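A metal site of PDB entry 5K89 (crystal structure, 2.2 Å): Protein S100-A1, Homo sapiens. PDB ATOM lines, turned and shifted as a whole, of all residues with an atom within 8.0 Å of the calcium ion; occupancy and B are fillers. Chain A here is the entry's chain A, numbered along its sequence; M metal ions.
ND2 of Asn 65 lies within hydrogen-bond range of OD1 of Asp 71, 3.3 Å away. The side-chain carboxylate (OE2) of Glu 74 is in hydrogen-bond range of the backbone NH (N) of Glu 64. The backbone NH (N) of Gly 66 lies close to the side-chain carboxylate (OD1) of Asp 63. The side-chain carboxylate of Asp 71 is in hydrogen-bond range of the backbone NH of Glu 74, at 3.1 Å. OD2 of Asp 71 sits close to N of Gln 73, 3.4 Å away. The side-chain carboxylate (OD2) of Asp 63 sits at hydrogen-bond distance from the backbone NH (N) of Gly 68 (2.7 Å). OD1 of Asp 67 is in salt-bridge range of NZ of Lys 28 (3.4 Å).
The calcium ion is bound by O of Glu 69 (2.3 Å), OD1 of Asn 65 (2.3 Å), OD2 of Asp 67 (2.4 Å), OE1 of Glu 74 (2.5 Å) and OD1 of Asp 63 (2.6 Å). The calcium ion has five donor atoms within binding distance. Slightly farther from the calcium ion lies OE2 of Glu 74 (3.0 Å). Slightly farther from the calcium ion lies the side-chain carboxylate (OD1) of Asp 67 (3.1 Å).
Merely in contact with the calcium ion: Asp 71 (3.7 Å). The nearest printed residue that does not touch the calcium ion is Val 70 (4.2 Å).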
ATOM      1  N   LYS A  28      24.766 -26.683  18.644  1.00  0.00           N
ATOM      2  CA  LYS A  28      23.415 -26.307  18.223  1.00  0.00           C
ATOM      3  C   LYS A  28      22.819 -25.326  19.232  1.00  0.00           C
ATOM      4  O   LYS A  28      22.975 -25.508  20.453  1.00  0.00           O
ATOM      5  CB  LYS A  28      22.487 -27.527  18.136  1.00  0.00           C
ATOM      6  CG  LYS A  28      22.829 -28.514  17.035  1.00  0.00           C
ATOM      7  CD  LYS A  28      22.193 -29.846  17.315  1.00  0.00           C
ATOM      8  CE  LYS A  28      21.113 -30.155  16.319  1.00  0.00           C
ATOM      9  NZ  LYS A  28      20.589 -31.526  16.518  1.00  0.00           N
ATOM     10  N   LEU A  29      22.126 -24.309  18.725  1.00  0.00           N
ATOM     11  CA  LEU A  29      21.459 -23.311  19.564  1.00  0.00           C
ATOM     12  C   LEU A  29      20.054 -23.796  19.938  1.00  0.00           C
ATOM     13  O   LEU A  29      19.238 -24.047  19.056  1.00  0.00           O
ATOM     14  CB  LEU A  29      21.356 -21.977  18.824  1.00  0.00           C
ATOM     15  CG  LEU A  29      22.622 -21.160  18.648  1.00  0.00           C
ATOM     16  CD1 LEU A  29      22.426 -20.089  17.606  1.00  0.00           C
ATOM     17  CD2 LEU A  29      22.991 -20.538  19.970  1.00  0.00           C
ATOM     18  N   MET A  59      12.941 -19.043  15.393  1.00  0.00           N
ATOM     19  CA  MET A  59      13.220 -20.477  15.462  1.00  0.00           C
ATOM     20  C   MET A  59      12.567 -21.231  14.305  1.00  0.00           C
ATOM     21  O   MET A  59      13.248 -21.910  13.532  1.00  0.00           O
ATOM     22  CB  MET A  59      12.743 -21.024  16.809  1.00  0.00           C
ATOM     23  CG  MET A  59      12.815 -22.521  16.917  1.00  0.00           C
ATOM     24  SD  MET A  59      14.494 -23.173  16.768  1.00  0.00           S
ATOM     25  CE  MET A  59      15.242 -22.514  18.252  1.00  0.00           C
ATOM     26  N   LEU A  62      14.253 -20.469  10.959  1.00  0.00           N
ATOM     27  CA  LEU A  62      15.612 -20.962  10.724  1.00  0.00           C
ATOM     28  C   LEU A  62      15.733 -22.467  10.804  1.00  0.00           C
ATOM     29  O   LEU A  62      16.651 -23.046  10.190  1.00  0.00           O
ATOM     30  CB  LEU A  62      16.603 -20.339  11.711  1.00  0.00           C
ATOM     31  CG  LEU A  62      16.955 -18.857  11.524  1.00  0.00           C
ATOM     32  CD1 LEU A  62      17.774 -18.334  12.686  1.00  0.00           C
ATOM     33  CD2 LEU A  62      17.660 -18.624  10.194  1.00  0.00           C
ATOM     34  N   ASP A  63      14.889 -23.128  11.605  1.00  0.00           N
ATOM     35  CA  ASP A  63      14.961 -24.571  11.791  1.00  0.00           C
ATOM     36  C   ASP A  63      14.521 -25.288  10.531  1.00  0.00           C
ATOM     37  O   ASP A  63      13.428 -25.861  10.436  1.00  0.00           O
ATOM     38  CB  ASP A  63      14.125 -25.029  12.976  1.00  0.00           C
ATOM     39  CG  ASP A  63      14.428 -26.452  13.371  1.00  0.00           C
ATOM     40  OD1 ASP A  63      15.397 -27.014  12.829  1.00  0.00           O
ATOM     41  OD2 ASP A  63      13.708 -27.024  14.212  1.00  0.00           O
ATOM     42  N   GLU A  64      15.401 -25.278   9.530  1.00  0.00           N
ATOM     43  CA  GLU A  64      15.065 -25.912   8.257  1.00  0.00           C
ATOM     44  C   GLU A  64      14.818 -27.408   8.441  1.00  0.00           C
ATOM     45  O   GLU A  64      13.869 -27.955   7.881  1.00  0.00           O
ATOM     46  CB  GLU A  64      16.185 -25.656   7.246  1.00  0.00           C
ATOM     47  CG  GLU A  64      15.771 -25.868   5.799  1.00  0.00           C
ATOM     48  CD  GLU A  64      16.892 -26.442   4.939  1.00  0.00           C
ATOM     49  OE1 GLU A  64      18.057 -26.390   5.382  1.00  0.00           O
ATOM     50  OE2 GLU A  64      16.597 -26.946   3.842  1.00  0.00           O
ATOM     51  N   ASN A  65      15.655 -28.083   9.235  1.00  0.00           N
ATOM     52  CA  ASN A  65      15.549 -29.545   9.348  1.00  0.00           C
ATOM     53  C   ASN A  65      14.500 -29.987  10.369  1.00  0.00           C
ATOM     54  O   ASN A  65      14.081 -31.148  10.321  1.00  0.00           O
ATOM     55  CB  ASN A  65      16.918 -30.178   9.642  1.00  0.00           C
ATOM     56  CG  ASN A  65      17.607 -29.552  10.831  1.00  0.00           C
ATOM     57  OD1 ASN A  65      16.988 -28.897  11.650  1.00  0.00           O
ATOM     58  ND2 ASN A  65      18.919 -29.777  10.925  1.00  0.00           N
ATOM     59  N   GLY A  66      14.127 -29.130  11.317  1.00  0.00           N
ATOM     60  CA  GLY A  66      12.986 -29.399  12.174  1.00  0.00           C
ATOM     61  C   GLY A  66      13.292 -30.234  13.401  1.00  0.00           C
ATOM     62  O   GLY A  66      12.485 -31.072  13.819  1.00  0.00           O
ATOM     63  N   ASP A  67      14.464 -30.005  13.984  1.00  0.00           N
ATOM     64  CA  ASP A  67      14.907 -30.700  15.180  1.00  0.00           C
ATOM     65  C   ASP A  67      14.738 -29.866  16.435  1.00  0.00           C
ATOM     66  O   ASP A  67      15.062 -30.340  17.534  1.00  0.00           O
ATOM     67  CB  ASP A  67      16.381 -31.109  15.005  1.00  0.00           C
ATOM     68  CG  ASP A  67      17.263 -29.939  14.591  1.00  0.00           C
ATOM     69  OD1 ASP A  67      18.428 -30.169  14.217  1.00  0.00           O
ATOM     70  OD2 ASP A  67      16.792 -28.791  14.584  1.00  0.00           O
ATOM     71  N   GLY A  68      14.253 -28.634  16.301  1.00  0.00           N
ATOM     72  CA  GLY A  68      14.023 -27.761  17.431  1.00  0.00           C
ATOM     73  C   GLY A  68      15.227 -26.958  17.876  1.00  0.00           C
ATOM     74  O   GLY A  68      15.122 -26.236  18.873  1.00  0.00           O
ATOM     75  N   GLU A  69      16.341 -27.009  17.145  1.00  0.00           N
ATOM     76  CA  GLU A  69      17.555 -26.273  17.464  1.00  0.00           C
ATOM     77  C   GLU A  69      18.183 -25.747  16.178  1.00  0.00           C
ATOM     78  O   GLU A  69      17.953 -26.293  15.100  1.00  0.00           O
ATOM     79  CB  GLU A  69      18.570 -27.157  18.229  1.00  0.00           C
ATOM     80  CG  GLU A  69      18.189 -27.537  19.674  1.00  0.00           C
ATOM     81  CD  GLU A  69      19.361 -28.125  20.464  1.00  0.00           C
ATOM     82  OE1 GLU A  69      19.356 -29.344  20.760  1.00  0.00           O
ATOM     83  OE2 GLU A  69      20.306 -27.374  20.789  1.00  0.00           O
ATOM     84  N   VAL A  70      18.932 -24.654  16.289  1.00  0.00           N
ATOM     85  CA  VAL A  70      19.624 -24.075  15.149  1.00  0.00           C
ATOM     86  C   VAL A  70      21.094 -24.486  15.203  1.00  0.00           C
ATOM     87  O   VAL A  70      21.813 -24.131  16.138  1.00  0.00           O
ATOM     88  CB  VAL A  70      19.520 -22.553  15.114  1.00  0.00           C
ATOM     89  CG1 VAL A  70      20.371 -22.003  13.958  1.00  0.00           C
ATOM     90  CG2 VAL A  70      18.066 -22.111  14.975  1.00  0.00           C
ATOM     91  N   ASP A  71      21.537 -25.191  14.161  1.00  0.00           N
ATOM     92  CA  ASP A  71      22.928 -25.557  14.000  1.00  0.00           C
ATOM     93  C   ASP A  71      23.655 -24.440  13.239  1.00  0.00           C
ATOM     94  O   ASP A  71      23.078 -23.381  12.958  1.00  0.00           O
ATOM     95  CB  ASP A  71      23.024 -26.903  13.291  1.00  0.00           C
ATOM     96  CG  ASP A  71      22.202 -26.943  12.008  1.00  0.00           C
ATOM     97  OD1 ASP A  71      21.397 -27.885  11.855  1.00  0.00           O
ATOM     98  OD2 ASP A  71      22.365 -26.053  11.159  1.00  0.00           O
ATOM     99  N   PHE A  72      24.937 -24.655  12.913  1.00  0.00           N
ATOM    100  CA  PHE A  72      25.705 -23.584  12.289  1.00  0.00           C
ATOM    101  C   PHE A  72      25.167 -23.265  10.879  1.00  0.00           C
ATOM    102  O   PHE A  72      24.887 -22.107  10.574  1.00  0.00           O
ATOM    103  CB  PHE A  72      27.202 -23.905  12.223  1.00  0.00           C
ATOM    104  CG  PHE A  72      28.060 -22.691  11.904  1.00  0.00           C
ATOM    105  CD1 PHE A  72      28.565 -22.490  10.628  1.00  0.00           C
ATOM    106  CD2 PHE A  72      28.287 -21.708  12.871  1.00  0.00           C
ATOM    107  CE1 PHE A  72      29.335 -21.354  10.325  1.00  0.00           C
ATOM    108  CE2 PHE A  72      29.058 -20.583  12.590  1.00  0.00           C
ATOM    109  CZ  PHE A  72      29.583 -20.406  11.310  1.00  0.00           C
ATOM    110  N   GLN A  73      24.998 -24.294  10.031  1.00  0.00           N
ATOM    111  CA  GLN A  73      24.538 -24.064   8.658  1.00  0.00           C
ATOM    112  C   GLN A  73      23.244 -23.255   8.609  1.00  0.00           C
ATOM    113  O   GLN A  73      23.001 -22.528   7.639  1.00  0.00           O
ATOM    114  CB  GLN A  73      24.366 -25.403   7.918  1.00  0.00           C
ATOM    115  CG  GLN A  73      23.272 -26.326   8.506  1.00  0.00           C
ATOM    116  CD  GLN A  73      23.112 -27.636   7.753  1.00  0.00           C
ATOM    117  OE1 GLN A  73      24.019 -28.073   7.033  1.00  0.00           O
ATOM    118  NE2 GLN A  73      21.964 -28.284   7.923  1.00  0.00           N
ATOM    119  N   GLU A  74      22.407 -23.369   9.634  1.00  0.00           N
ATOM    120  CA  GLU A  74      21.155 -22.641   9.644  1.00  0.00           C
ATOM    121  C   GLU A  74      21.314 -21.249  10.201  1.00  0.00           C
ATOM    122  O   GLU A  74      20.551 -20.336   9.843  1.00  0.00           O
ATOM    123  CB  GLU A  74      20.104 -23.406  10.450  1.00  0.00           C
ATOM    124  CG  GLU A  74      19.695 -24.718   9.799  1.00  0.00           C
ATOM    125  CD  GLU A  74      18.883 -25.609  10.712  1.00  0.00           C
ATOM    126  OE1 GLU A  74      18.835 -25.311  11.923  1.00  0.00           O
ATOM    127  OE2 GLU A  74      18.296 -26.600  10.217  1.00  0.00           O
ATOM    128  N   TYR A  75      22.262 -21.081  11.122  1.00  0.00           N
ATOM    129  CA  TYR A  75      22.570 -19.774  11.685  1.00  0.00           C
ATOM    130  C   TYR A  75      23.248 -18.869  10.656  1.00  0.00           C
ATOM    131  O   TYR A  75      23.103 -17.644  10.722  1.00  0.00           O
ATOM    132  CB  TYR A  75      23.440 -19.968  12.917  1.00  0.00           C
ATOM    133  CG  TYR A  75      24.396 -18.854  13.234  1.00  0.00           C
ATOM    134  CD1 TYR A  75      24.017 -17.791  14.025  1.00  0.00           C
ATOM    135  CD2 TYR A  75      25.693 -18.888  12.747  1.00  0.00           C
ATOM    136  CE1 TYR A  75      24.926 -16.792  14.330  1.00  0.00           C
ATOM    137  CE2 TYR A  75      26.594 -17.889  13.029  1.00  0.00           C
ATOM    138  CZ  TYR A  75      26.223 -16.850  13.823  1.00  0.00           C
ATOM    139  OH  TYR A  75      27.163 -15.869  14.090  1.00  0.00           O
HETATM  140 CA    CA M   1      17.926 -27.304  13.078  1.00  0.00          CA
